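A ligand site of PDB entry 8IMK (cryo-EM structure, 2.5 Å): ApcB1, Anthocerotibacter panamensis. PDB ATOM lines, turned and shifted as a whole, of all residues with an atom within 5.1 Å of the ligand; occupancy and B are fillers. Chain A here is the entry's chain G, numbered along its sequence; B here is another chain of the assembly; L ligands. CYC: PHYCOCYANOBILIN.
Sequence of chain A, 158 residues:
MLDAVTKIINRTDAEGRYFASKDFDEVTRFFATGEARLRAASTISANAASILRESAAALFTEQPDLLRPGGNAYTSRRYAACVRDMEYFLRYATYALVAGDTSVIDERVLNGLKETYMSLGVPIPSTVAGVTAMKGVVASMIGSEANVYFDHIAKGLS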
ATOM      1  N   LEU A  59      19.134  28.011  34.156  1.00  0.00           N
ATOM      2  CA  LEU A  59      19.473  27.887  32.740  1.00  0.00           C
ATOM      3  C   LEU A  59      19.765  29.248  32.126  1.00  0.00           C
ATOM      4  O   LEU A  59      20.758  29.417  31.406  1.00  0.00           O
ATOM      5  CB  LEU A  59      18.353  27.193  31.974  1.00  0.00           C
ATOM      6  CG  LEU A  59      18.485  27.295  30.452  1.00  0.00           C
ATOM      7  CD1 LEU A  59      19.715  26.547  29.956  1.00  0.00           C
ATOM      8  CD2 LEU A  59      17.230  26.840  29.734  1.00  0.00           C
ATOM      9  N   LEU A  66      20.239  32.896  25.064  1.00  0.00           N
ATOM     10  CA  LEU A  66      18.972  32.310  24.667  1.00  0.00           C
ATOM     11  C   LEU A  66      17.860  33.340  24.704  1.00  0.00           C
ATOM     12  O   LEU A  66      17.002  33.386  23.819  1.00  0.00           O
ATOM     13  CB  LEU A  66      18.654  31.123  25.579  1.00  0.00           C
ATOM     14  CG  LEU A  66      19.488  29.861  25.359  1.00  0.00           C
ATOM     15  CD1 LEU A  66      19.077  28.780  26.322  1.00  0.00           C
ATOM     16  CD2 LEU A  66      19.372  29.380  23.935  1.00  0.00           C
ATOM     17  N   ASN A  72      16.783  31.518  20.747  1.00  0.00           N
ATOM     18  CA  ASN A  72      15.683  30.577  20.571  1.00  0.00           C
ATOM     19  C   ASN A  72      14.624  30.730  21.655  1.00  0.00           C
ATOM     20  O   ASN A  72      13.493  30.271  21.484  1.00  0.00           O
ATOM     21  CB  ASN A  72      16.212  29.149  20.526  1.00  0.00           C
ATOM     22  CG  ASN A  72      15.177  28.158  20.036  1.00  0.00           C
ATOM     23  OD1 ASN A  72      14.888  27.174  20.701  1.00  0.00           O
ATOM     24  ND2 ASN A  72      14.604  28.429  18.871  1.00  0.00           N
ATOM     25  N   ALA A  73      14.965  31.350  22.777  1.00  0.00           N
ATOM     26  CA  ALA A  73      13.997  31.617  23.825  1.00  0.00           C
ATOM     27  C   ALA A  73      13.527  33.068  23.830  1.00  0.00           C
ATOM     28  O   ALA A  73      12.858  33.477  24.777  1.00  0.00           O
ATOM     29  CB  ALA A  73      14.580  31.251  25.188  1.00  0.00           C
ATOM     30  N   ARG A  77       6.167  33.858  23.684  1.00  0.00           N
ATOM     31  CA  ARG A  77       5.690  32.532  23.305  1.00  0.00           C
ATOM     32  C   ARG A  77       6.814  31.495  23.362  1.00  0.00           C
ATOM     33  O   ARG A  77       6.618  30.387  23.869  1.00  0.00           O
ATOM     34  CB  ARG A  77       5.072  32.574  21.913  1.00  0.00           C
ATOM     35  CG  ARG A  77       4.557  31.241  21.443  1.00  0.00           C
ATOM     36  CD  ARG A  77       4.329  31.236  19.943  1.00  0.00           C
ATOM     37  NE  ARG A  77       5.559  31.415  19.184  1.00  0.00           N
ATOM     38  CZ  ARG A  77       6.316  30.415  18.732  1.00  0.00           C
ATOM     39  NH1 ARG A  77       5.964  29.169  18.970  1.00  0.00           N
ATOM     40  NH2 ARG A  77       7.415  30.680  18.043  1.00  0.00           N
ATOM     41  N   ARG A  78       7.990  31.842  22.855  1.00  0.00           N
ATOM     42  CA  ARG A  78       9.078  30.876  22.839  1.00  0.00           C
ATOM     43  C   ARG A  78       9.613  30.623  24.249  1.00  0.00           C
ATOM     44  O   ARG A  78       9.991  29.500  24.581  1.00  0.00           O
ATOM     45  CB  ARG A  78      10.191  31.327  21.900  1.00  0.00           C
ATOM     46  CG  ARG A  78       9.875  31.020  20.456  1.00  0.00           C
ATOM     47  CD  ARG A  78      11.086  31.069  19.574  1.00  0.00           C
ATOM     48  NE  ARG A  78      11.040  32.188  18.633  1.00  0.00           N
ATOM     49  CZ  ARG A  78      11.940  33.156  18.584  1.00  0.00           C
ATOM     50  NH1 ARG A  78      12.964  33.142  19.416  1.00  0.00           N
ATOM     51  NH2 ARG A  78      11.819  34.125  17.701  1.00  0.00           N
ATOM     52  N   ALA A  81       7.189  28.304  25.801  1.00  0.00           N
ATOM     53  CA  ALA A  81       7.392  26.937  25.334  1.00  0.00           C
ATOM     54  C   ALA A  81       8.624  26.297  25.950  1.00  0.00           C
ATOM     55  O   ALA A  81       8.618  25.094  26.246  1.00  0.00           O
ATOM     56  CB  ALA A  81       7.498  26.936  23.807  1.00  0.00           C
ATOM     57  N   CYS A  82       9.697  27.069  26.121  1.00  0.00           N
ATOM     58  CA  CYS A  82      10.875  26.543  26.804  1.00  0.00           C
ATOM     59  C   CYS A  82      10.542  26.095  28.229  1.00  0.00           C
ATOM     60  O   CYS A  82      10.878  24.969  28.632  1.00  0.00           O
ATOM     61  CB  CYS A  82      11.968  27.612  26.809  1.00  0.00           C
ATOM     62  SG  CYS A  82      13.374  27.314  27.867  1.00  0.00           S
ATOM     63  N   ARG A  84       7.645  25.379  29.373  1.00  0.00           N
ATOM     64  CA  ARG A  84       6.692  24.281  29.250  1.00  0.00           C
ATOM     65  C   ARG A  84       7.400  22.957  28.986  1.00  0.00           C
ATOM     66  O   ARG A  84       7.021  21.914  29.520  1.00  0.00           O
ATOM     67  CB  ARG A  84       5.691  24.634  28.156  1.00  0.00           C
ATOM     68  CG  ARG A  84       4.445  23.790  28.044  1.00  0.00           C
ATOM     69  CD  ARG A  84       4.703  22.527  27.262  1.00  0.00           C
ATOM     70  NE  ARG A  84       5.578  22.762  26.109  1.00  0.00           N
ATOM     71  CZ  ARG A  84       5.156  23.140  24.909  1.00  0.00           C
ATOM     72  NH1 ARG A  84       3.867  23.335  24.671  1.00  0.00           N
ATOM     73  NH2 ARG A  84       6.029  23.325  23.938  1.00  0.00           N
ATOM     74  N   ASP A  85       8.435  22.973  28.150  1.00  0.00           N
ATOM     75  CA  ASP A  85       9.246  21.779  27.927  1.00  0.00           C
ATOM     76  C   ASP A  85       9.915  21.338  29.220  1.00  0.00           C
ATOM     77  O   ASP A  85      10.005  20.133  29.505  1.00  0.00           O
ATOM     78  CB  ASP A  85      10.306  22.054  26.863  1.00  0.00           C
ATOM     79  CG  ASP A  85       9.762  21.952  25.467  1.00  0.00           C
ATOM     80  OD1 ASP A  85       8.537  21.830  25.307  1.00  0.00           O
ATOM     81  OD2 ASP A  85      10.562  22.004  24.512  1.00  0.00           O
ATOM     82  N   MET A  86      10.400  22.293  29.996  1.00  0.00           N
ATOM     83  CA  MET A  86      11.019  21.931  31.272  1.00  0.00           C
ATOM     84  C   MET A  86       9.992  21.355  32.247  1.00  0.00           C
ATOM     85  O   MET A  86      10.299  20.455  33.028  1.00  0.00           O
ATOM     86  CB  MET A  86      11.738  23.145  31.834  1.00  0.00           C
ATOM     87  CG  MET A  86      13.140  23.270  31.283  1.00  0.00           C
ATOM     88  SD  MET A  86      14.051  24.706  31.879  1.00  0.00           S
ATOM     89  CE  MET A  86      14.471  24.149  33.516  1.00  0.00           C
ATOM     90  N   TYR A  88       7.413  19.567  31.185  1.00  0.00           N
ATOM     91  CA  TYR A  88       7.342  18.203  30.674  1.00  0.00           C
ATOM     92  C   TYR A  88       8.397  17.324  31.322  1.00  0.00           C
ATOM     93  O   TYR A  88       8.094  16.222  31.809  1.00  0.00           O
ATOM     94  CB  TYR A  88       7.571  18.164  29.165  1.00  0.00           C
ATOM     95  CG  TYR A  88       6.439  18.569  28.279  1.00  0.00           C
ATOM     96  CD1 TYR A  88       5.119  18.373  28.644  1.00  0.00           C
ATOM     97  CD2 TYR A  88       6.695  19.099  27.022  1.00  0.00           C
ATOM     98  CE1 TYR A  88       4.093  18.736  27.814  1.00  0.00           C
ATOM     99  CE2 TYR A  88       5.694  19.460  26.195  1.00  0.00           C
ATOM    100  CZ  TYR A  88       4.388  19.273  26.573  1.00  0.00           C
ATOM    101  OH  TYR A  88       3.390  19.647  25.727  1.00  0.00           O
ATOM    102  N   PHE A  89       9.643  17.790  31.308  1.00  0.00           N
ATOM    103  CA  PHE A  89      10.737  16.978  31.818  1.00  0.00           C
ATOM    104  C   PHE A  89      10.568  16.675  33.292  1.00  0.00           C
ATOM    105  O   PHE A  89      10.775  15.539  33.730  1.00  0.00           O
ATOM    106  CB  PHE A  89      12.078  17.660  31.544  1.00  0.00           C
ATOM    107  CG  PHE A  89      12.354  17.874  30.096  1.00  0.00           C
ATOM    108  CD1 PHE A  89      11.865  16.988  29.154  1.00  0.00           C
ATOM    109  CD2 PHE A  89      13.109  18.936  29.671  1.00  0.00           C
ATOM    110  CE1 PHE A  89      12.124  17.169  27.821  1.00  0.00           C
ATOM    111  CE2 PHE A  89      13.373  19.120  28.330  1.00  0.00           C
ATOM    112  CZ  PHE A  89      12.870  18.240  27.406  1.00  0.00           C
ATOM    113  N   TYR A  92       7.587  14.119  33.831  1.00  0.00           N
ATOM    114  CA  TYR A  92       7.858  12.770  33.365  1.00  0.00           C
ATOM    115  C   TYR A  92       8.991  12.112  34.134  1.00  0.00           C
ATOM    116  O   TYR A  92       8.993  10.886  34.326  1.00  0.00           O
ATOM    117  CB  TYR A  92       8.121  12.782  31.872  1.00  0.00           C
ATOM    118  CG  TYR A  92       6.826  12.756  31.109  1.00  0.00           C
ATOM    119  CD1 TYR A  92       6.065  11.607  31.046  1.00  0.00           C
ATOM    120  CD2 TYR A  92       6.334  13.893  30.505  1.00  0.00           C
ATOM    121  CE1 TYR A  92       4.873  11.590  30.380  1.00  0.00           C
ATOM    122  CE2 TYR A  92       5.152  13.886  29.837  1.00  0.00           C
ATOM    123  CZ  TYR A  92       4.415  12.736  29.777  1.00  0.00           C
ATOM    124  OH  TYR A  92       3.229  12.722  29.104  1.00  0.00           O
ATOM    125  N   ARG A 108       7.058   8.638  26.027  1.00  0.00           N
ATOM    126  CA  ARG A 108       6.286   9.876  26.029  1.00  0.00           C
ATOM    127  C   ARG A 108       7.149  11.088  25.743  1.00  0.00           C
ATOM    128  O   ARG A 108       6.669  12.068  25.164  1.00  0.00           O
ATOM    129  CB  ARG A 108       5.556  10.040  27.361  1.00  0.00           C
ATOM    130  CG  ARG A 108       4.557   8.936  27.671  1.00  0.00           C
ATOM    131  CD  ARG A 108       3.239   9.197  26.973  1.00  0.00           C
ATOM    132  NE  ARG A 108       2.519   7.950  26.699  1.00  0.00           N
ATOM    133  CZ  ARG A 108       1.650   7.390  27.535  1.00  0.00           C
ATOM    134  NH1 ARG A 108       1.388   7.962  28.702  1.00  0.00           N
ATOM    135  NH2 ARG A 108       1.048   6.267  27.210  1.00  0.00           N
ATOM    136  N   VAL A 109       8.422  11.040  26.124  1.00  0.00           N
ATOM    137  CA  VAL A 109       9.295  12.199  26.053  1.00  0.00           C
ATOM    138  C   VAL A 109      10.281  12.101  24.890  1.00  0.00           C
ATOM    139  O   VAL A 109      10.331  12.982  24.039  1.00  0.00           O
ATOM    140  CB  VAL A 109      10.033  12.384  27.394  1.00  0.00           C
ATOM    141  CG1 VAL A 109      11.060  13.486  27.291  1.00  0.00           C
ATOM    142  CG2 VAL A 109       9.050  12.683  28.482  1.00  0.00           C
ATOM    143  N   LEU A 113      11.762  13.271  19.781  1.00  0.00           N
ATOM    144  CA  LEU A 113      12.051  14.605  20.288  1.00  0.00           C
ATOM    145  C   LEU A 113      13.226  15.242  19.547  1.00  0.00           C
ATOM    146  O   LEU A 113      13.200  16.432  19.237  1.00  0.00           O
ATOM    147  CB  LEU A 113      12.334  14.559  21.781  1.00  0.00           C
ATOM    148  CG  LEU A 113      12.606  15.900  22.456  1.00  0.00           C
ATOM    149  CD1 LEU A 113      11.513  16.879  22.085  1.00  0.00           C
ATOM    150  CD2 LEU A 113      12.698  15.736  23.955  1.00  0.00           C
ATOM    151  N   THR A 116      12.199  16.460  16.174  1.00  0.00           N
ATOM    152  CA  THR A 116      11.321  17.619  16.289  1.00  0.00           C
ATOM    153  C   THR A 116      12.097  18.874  16.678  1.00  0.00           C
ATOM    154  O   THR A 116      11.769  19.972  16.232  1.00  0.00           O
ATOM    155  CB  THR A 116      10.217  17.335  17.307  1.00  0.00           C
ATOM    156  OG1 THR A 116       9.622  16.067  17.009  1.00  0.00           O
ATOM    157  CG2 THR A 116       9.150  18.405  17.238  1.00  0.00           C
ATOM    158  N   TYR A 117      13.139  18.725  17.497  1.00  0.00           N
ATOM    159  CA  TYR A 117      13.947  19.883  17.847  1.00  0.00           C
ATOM    160  C   TYR A 117      14.847  20.318  16.696  1.00  0.00           C
ATOM    161  O   TYR A 117      15.097  21.517  16.524  1.00  0.00           O
ATOM    162  CB  TYR A 117      14.785  19.599  19.096  1.00  0.00           C
ATOM    163  CG  TYR A 117      14.028  19.727  20.385  1.00  0.00           C
ATOM    164  CD1 TYR A 117      12.781  20.320  20.422  1.00  0.00           C
ATOM    165  CD2 TYR A 117      14.587  19.325  21.593  1.00  0.00           C
ATOM    166  CE1 TYR A 117      12.093  20.464  21.600  1.00  0.00           C
ATOM    167  CE2 TYR A 117      13.911  19.471  22.779  1.00  0.00           C
ATOM    168  CZ  TYR A 117      12.675  20.044  22.779  1.00  0.00           C
ATOM    169  OH  TYR A 117      12.003  20.176  23.963  1.00  0.00           O
ATOM    170  N   LEU A 120      12.437  22.171  14.517  1.00  0.00           N
ATOM    171  CA  LEU A 120      12.031  23.435  15.126  1.00  0.00           C
ATOM    172  C   LEU A 120      13.196  24.407  15.231  1.00  0.00           C
ATOM    173  O   LEU A 120      13.010  25.627  15.126  1.00  0.00           O
ATOM    174  CB  LEU A 120      11.449  23.189  16.508  1.00  0.00           C
ATOM    175  CG  LEU A 120      10.052  22.592  16.611  1.00  0.00           C
ATOM    176  CD1 LEU A 120       9.806  22.131  18.026  1.00  0.00           C
ATOM    177  CD2 LEU A 120       9.002  23.595  16.176  1.00  0.00           C
ATOM    178  N   VAL A 122      15.308  24.117  18.048  1.00  0.00           N
ATOM    179  CA  VAL A 122      15.652  24.182  19.472  1.00  0.00           C
ATOM    180  C   VAL A 122      17.049  23.599  19.665  1.00  0.00           C
ATOM    181  O   VAL A 122      17.292  22.441  19.289  1.00  0.00           O
ATOM    182  CB  VAL A 122      14.621  23.422  20.315  1.00  0.00           C
ATOM    183  CG1 VAL A 122      15.049  23.391  21.773  1.00  0.00           C
ATOM    184  CG2 VAL A 122      13.249  24.044  20.178  1.00  0.00           C
ATOM    185  N   PRO A 123      17.992  24.343  20.230  1.00  0.00           N
ATOM    186  CA  PRO A 123      19.346  23.809  20.462  1.00  0.00           C
ATOM    187  C   PRO A 123      19.328  22.681  21.482  1.00  0.00           C
ATOM    188  O   PRO A 123      18.903  22.871  22.627  1.00  0.00           O
ATOM    189  CB  PRO A 123      20.137  25.022  20.972  1.00  0.00           C
ATOM    190  CG  PRO A 123      19.117  26.001  21.403  1.00  0.00           C
ATOM    191  CD  PRO A 123      17.899  25.777  20.581  1.00  0.00           C
ATOM    192  N   SER A 126      21.630  23.302  24.737  1.00  0.00           N
ATOM    193  CA  SER A 126      21.023  24.225  25.688  1.00  0.00           C
ATOM    194  C   SER A 126      19.863  23.554  26.427  1.00  0.00           C
ATOM    195  O   SER A 126      19.672  23.781  27.628  1.00  0.00           O
ATOM    196  CB  SER A 126      20.562  25.481  24.973  1.00  0.00           C
ATOM    197  OG  SER A 126      21.588  25.986  24.134  1.00  0.00           O
ATOM    198  N   THR A 127      19.087  22.724  25.728  1.00  0.00           N
ATOM    199  CA  THR A 127      18.035  21.964  26.381  1.00  0.00           C
ATOM    200  C   THR A 127      18.617  20.982  27.391  1.00  0.00           C
ATOM    201  O   THR A 127      18.058  20.776  28.476  1.00  0.00           O
ATOM    202  CB  THR A 127      17.193  21.225  25.344  1.00  0.00           C
ATOM    203  OG1 THR A 127      16.850  22.138  24.292  1.00  0.00           O
ATOM    204  CG2 THR A 127      15.918  20.704  25.960  1.00  0.00           C
ATOM    205  N   GLY A 130      19.531  22.910  30.447  1.00  0.00           N
ATOM    206  CA  GLY A 130      18.340  23.103  31.256  1.00  0.00           C
ATOM    207  C   GLY A 130      17.962  21.859  32.031  1.00  0.00           C
ATOM    208  O   GLY A 130      17.568  21.933  33.203  1.00  0.00           O
ATOM    209  N   ARG B  13       3.273  25.228  16.362  1.00  0.00           N
ATOM    210  CA  ARG B  13       2.146  25.822  17.072  1.00  0.00           C
ATOM    211  C   ARG B  13       2.351  27.305  17.339  1.00  0.00           C
ATOM    212  O   ARG B  13       1.929  27.814  18.375  1.00  0.00           O
ATOM    213  CB  ARG B  13       1.911  25.073  18.376  1.00  0.00           C
ATOM    214  CG  ARG B  13       1.746  23.592  18.187  1.00  0.00           C
ATOM    215  CD  ARG B  13       1.046  22.963  19.349  1.00  0.00           C
ATOM    216  NE  ARG B  13      -0.334  23.390  19.564  1.00  0.00           N
ATOM    217  CZ  ARG B  13      -1.344  23.053  18.763  1.00  0.00           C
ATOM    218  NH1 ARG B  13      -1.139  22.281  17.712  1.00  0.00           N
ATOM    219  NH2 ARG B  13      -2.573  23.469  19.050  1.00  0.00           N
ATOM    220  N   ARG B  14       2.987  28.009  16.399  1.00  0.00           N
ATOM    221  CA  ARG B  14       3.466  29.355  16.674  1.00  0.00           C
ATOM    222  C   ARG B  14       2.336  30.365  16.753  1.00  0.00           C
ATOM    223  O   ARG B  14       2.554  31.517  17.134  1.00  0.00           O
ATOM    224  CB  ARG B  14       4.486  29.761  15.605  1.00  0.00           C
ATOM    225  CG  ARG B  14       5.751  28.916  15.626  1.00  0.00           C
ATOM    226  CD  ARG B  14       6.676  29.252  14.482  1.00  0.00           C
ATOM    227  NE  ARG B  14       7.948  28.536  14.580  1.00  0.00           N
ATOM    228  CZ  ARG B  14       8.432  27.743  13.631  1.00  0.00           C
ATOM    229  NH1 ARG B  14       9.589  27.122  13.813  1.00  0.00           N
ATOM    230  NH2 ARG B  14       7.764  27.575  12.494  1.00  0.00           N
ATOM    231  N   SER B  21      -0.410  19.593  27.806  1.00  0.00           N
ATOM    232  CA  SER B  21      -0.702  18.298  27.211  1.00  0.00           C
ATOM    233  C   SER B  21       0.385  17.894  26.230  1.00  0.00           C
ATOM    234  O   SER B  21       1.076  18.732  25.641  1.00  0.00           O
ATOM    235  CB  SER B  21      -2.061  18.334  26.503  1.00  0.00           C
ATOM    236  OG  SER B  21      -1.942  18.909  25.208  1.00  0.00           O
ATOM    237  N   ARG B  22       0.563  16.584  26.057  1.00  0.00           N
ATOM    238  CA  ARG B  22       1.481  16.099  25.034  1.00  0.00           C
ATOM    239  C   ARG B  22       0.975  16.488  23.655  1.00  0.00           C
ATOM    240  O   ARG B  22      -0.212  16.365  23.357  1.00  0.00           O
ATOM    241  CB  ARG B  22       1.644  14.582  25.101  1.00  0.00           C
ATOM    242  CG  ARG B  22       2.656  14.101  26.106  1.00  0.00           C
ATOM    243  CD  ARG B  22       2.799  12.601  26.016  1.00  0.00           C
ATOM    244  NE  ARG B  22       3.784  12.222  25.001  1.00  0.00           N
ATOM    245  CZ  ARG B  22       3.469  11.806  23.782  1.00  0.00           C
ATOM    246  NH1 ARG B  22       2.199  11.732  23.420  1.00  0.00           N
ATOM    247  NH2 ARG B  22       4.423  11.493  22.921  1.00  0.00           N
ATOM    248  N   GLU B  23       1.892  16.956  22.818  1.00  0.00           N
ATOM    249  CA  GLU B  23       1.509  17.597  21.577  1.00  0.00           C
ATOM    250  C   GLU B  23       2.435  17.182  20.433  1.00  0.00           C
ATOM    251  O   GLU B  23       2.165  17.502  19.275  1.00  0.00           O
ATOM    252  CB  GLU B  23       1.553  19.107  21.796  1.00  0.00           C
ATOM    253  CG  GLU B  23       1.136  19.966  20.649  1.00  0.00           C
ATOM    254  CD  GLU B  23      -0.327  19.808  20.304  1.00  0.00           C
ATOM    255  OE1 GLU B  23      -1.123  19.445  21.185  1.00  0.00           O
ATOM    256  OE2 GLU B  23      -0.694  20.068  19.134  1.00  0.00           O
ATOM    257  N   ILE B  24       3.492  16.429  20.739  1.00  0.00           N
ATOM    258  CA  ILE B  24       4.595  16.236  19.808  1.00  0.00           C
ATOM    259  C   ILE B  24       4.156  15.471  18.567  1.00  0.00           C
ATOM    260  O   ILE B  24       4.669  15.696  17.470  1.00  0.00           O
ATOM    261  CB  ILE B  24       5.775  15.542  20.519  1.00  0.00           C
ATOM    262  CG1 ILE B  24       7.008  15.552  19.638  1.00  0.00           C
ATOM    263  CG2 ILE B  24       5.398  14.129  20.931  1.00  0.00           C
ATOM    264  CD1 ILE B  24       8.292  15.505  20.417  1.00  0.00           C
ATOM    265  N   VAL B  27       2.517  17.533  15.849  1.00  0.00           N
ATOM    266  CA  VAL B  27       3.358  18.612  15.336  1.00  0.00           C
ATOM    267  C   VAL B  27       4.256  18.094  14.224  1.00  0.00           C
ATOM    268  O   VAL B  27       4.300  18.650  13.124  1.00  0.00           O
ATOM    269  CB  VAL B  27       4.185  19.246  16.474  1.00  0.00           C
ATOM    270  CG1 VAL B  27       5.260  20.142  15.913  1.00  0.00           C
ATOM    271  CG2 VAL B  27       3.281  20.000  17.430  1.00  0.00           C
HETATM  272  CHA CYC L   1       8.221  24.045  21.128  1.00  0.00           C
HETATM  273  NA  CYC L   1       8.629  21.739  22.240  1.00  0.00           N
HETATM  274  C1A CYC L   1       8.074  22.497  21.317  1.00  0.00           C
HETATM  275  C2A CYC L   1       7.310  21.702  20.488  1.00  0.00           C
HETATM  276  C3A CYC L   1       7.434  20.400  20.974  1.00  0.00           C
HETATM  277  C4A CYC L   1       8.264  20.475  22.085  1.00  0.00           C
HETATM  278  CMA CYC L   1       6.746  19.188  20.332  1.00  0.00           C
HETATM  279  CAA CYC L   1       6.489  22.171  19.267  1.00  0.00           C
HETATM  280  CBA CYC L   1       4.975  22.370  19.636  1.00  0.00           C
HETATM  281  CGA CYC L   1       4.737  23.591  20.629  1.00  0.00           C
HETATM  282  O1A CYC L   1       5.192  24.741  20.337  1.00  0.00           O
HETATM  283  O2A CYC L   1       4.096  23.400  21.716  1.00  0.00           O
HETATM  284  CHB CYC L   1       8.775  19.287  23.060  1.00  0.00           C
HETATM  285  NB  CYC L   1       6.468  18.219  23.200  1.00  0.00           N
HETATM  286  C1B CYC L   1       7.736  18.281  23.505  1.00  0.00           C
HETATM  287  C2B CYC L   1       8.008  17.242  24.337  1.00  0.00           C
HETATM  288  C3B CYC L   1       6.834  16.541  24.514  1.00  0.00           C
HETATM  289  C4B CYC L   1       5.887  17.192  23.767  1.00  0.00           C
HETATM  290  CMB CYC L   1       9.369  16.933  24.959  1.00  0.00           C
HETATM  291  CAB CYC L   1       6.643  15.257  25.412  1.00  0.00           C
HETATM  292  CBB CYC L   1       5.839  15.500  26.650  1.00  0.00           C
HETATM  293  OB  CYC L   1       4.500  16.819  23.645  1.00  0.00           O
HETATM  294  NC  CYC L   1      14.136  26.092  23.311  1.00  0.00           N
HETATM  295  C1C CYC L   1      15.349  26.759  23.952  1.00  0.00           C
HETATM  296  C2C CYC L   1      15.534  25.993  25.381  1.00  0.00           C
HETATM  297  C3C CYC L   1      14.759  24.991  25.274  1.00  0.00           C
HETATM  298  C4C CYC L   1      13.497  25.666  24.388  1.00  0.00           C
HETATM  299  CMC CYC L   1      17.090  25.603  25.487  1.00  0.00           C
HETATM  300  CAC CYC L   1      14.170  24.385  26.620  1.00  0.00           C
HETATM  301  CBC CYC L   1      15.102  24.242  27.846  1.00  0.00           C
HETATM  302  OC  CYC L   1      15.123  27.976  24.123  1.00  0.00           O
HETATM  303  CHD CYC L   1      12.410  24.659  24.108  1.00  0.00           C
HETATM  304  ND  CYC L   1      10.338  24.193  22.700  1.00  0.00           N
HETATM  305  C1D CYC L   1      11.275  25.065  23.056  1.00  0.00           C
HETATM  306  C2D CYC L   1      11.012  26.269  22.341  1.00  0.00           C
HETATM  307  C3D CYC L   1       9.888  26.022  21.574  1.00  0.00           C
HETATM  308  C4D CYC L   1       9.498  24.717  21.827  1.00  0.00           C
HETATM  309  CMD CYC L   1      11.723  27.660  22.309  1.00  0.00           C
HETATM  310  CAD CYC L   1       9.204  27.004  20.620  1.00  0.00           C
HETATM  311  CBD CYC L   1       9.857  26.935  19.233  1.00  0.00           C
HETATM  312  CGD CYC L   1       9.060  27.734  18.188  1.00  0.00           C
HETATM  313  O1D CYC L   1       9.665  28.415  17.320  1.00  0.00           O
HETATM  314  O2D CYC L   1       7.818  27.691  18.209  1.00  0.00           O
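OE2 of Glu 23 of chain B is in salt-bridge range of NH1 of Arg 13 of chain B. The guanidinium group (NE) of Arg 84 is in salt-bridge range of the side-chain carboxylate (OD1) of Asp 85, at 3.2 Å. The backbone carbonyl oxygen of Arg 108 is in hydrogen-bond range of the guanidinium group of Arg 22 of chain B, at 2.9 Å. The backbone NH (N) of Val 122 lies within hydrogen-bond range of the backbone carbonyl oxygen (O) of Tyr 117, 3.0 Å away. O of Ser 21 of chain B is in hydrogen-bond range of OH of Tyr 88. The backbone carbonyl oxygen (O) of Leu 66 is in hydrogen-bond range of the backbone NH (N) of Ala 73 (3.1 Å). OG1 of Thr 127 is in hydrogen-bond range of O of Pro 123 (2.7 Å).
NH1 of Arg 77 is in salt-bridge range of O2D of the ligand (2.5 Å). OB of the ligand is in hydrogen-bond range of N of Glu 23 of chain B (2.7 Å). The side-chain carboxylate (OD2) of Asp 85 lies within hydrogen-bond range of a nitrogen (ND) of the ligand (2.9 Å). NC of the ligand sits at hydrogen-bond distance from OD1 of Asn 72, at 2.9 Å. O2A of the ligand is in salt-bridge range of NH2 of Arg 84. The backbone NH (N) of Ile 24 of chain B sits at hydrogen-bond distance from an oxygen (OB) of the ligand, 3.1 Å away. An oxygen (O1D) of the ligand is in salt-bridge range of the guanidinium group (NE) of Arg 14 of chain B (3.2 Å).
CD2 of Leu 59 touches CBC of the ligand, 3.9 Å away. Leu 66 touches the ligand (CD1 to CMC, 3.8 Å). CB of Ala 73 touches OC of the ligand, 3.5 Å away. O of Arg 78 touches CMD of the ligand, 3.4 Å away. Ala 81 touches the ligand (CB to C3D, 3.4 Å). Cys 82 touches the ligand (SG to CAC, 3.3 Å). CE2 of Tyr 88 touches C4B of the ligand, at 3.3 Å. Phe 89 touches the ligand (CE1 to CMB, 3.98 Å). CE2 of Tyr 92 touches CBB of the ligand, 3.6 Å away. O of Arg 108 touches CAB of the ligand, at 3.2 Å. Leu 113 touches the ligand. Thr 116 touches the ligand (CG2 to CMA, 3.996 Å). Tyr 117 touches the ligand. Leu 120 touches the ligand (CD1 to C2A, 3.5 Å). Val 122 touches the ligand. Ser 126 touches the ligand (CB to CMC, 3.5 Å). Thr 127 touches the ligand. CG of Arg 13 of chain B touches CBA of the ligand, 3.7 Å away. Arg 22 of chain B touches the ligand (CA to OB, 3.4 Å). CG2 of Val 27 of chain B touches CBA of the ligand (3.7 Å). Hydrophobic or aromatic side chains that line the ligand: Leu 59, Leu 66, Ala 73, Ala 81, Tyr 88, Phe 89, Tyr 92, Leu 113, Tyr 117, Leu 120, Val 122, Ile 24 of chain B and Val 27 of chain B. Within 4 Å of the ligand: Leu 59, Leu 66, Asn 72, Ala 73, Arg 77, Arg 78, Ala 81, Cys 82, Arg 84, Asp 85, Tyr 88, Phe 89, Tyr 92, Arg 108, Leu 113, Thr 116, Tyr 117, Leu 120, Val 122, Ser 126, Thr 127, Arg 13 of chain B, Arg 14 of chain B, Arg 22 of chain B, Glu 23 of chain B, Ile 24 of chain B and Val 27 of chain B.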
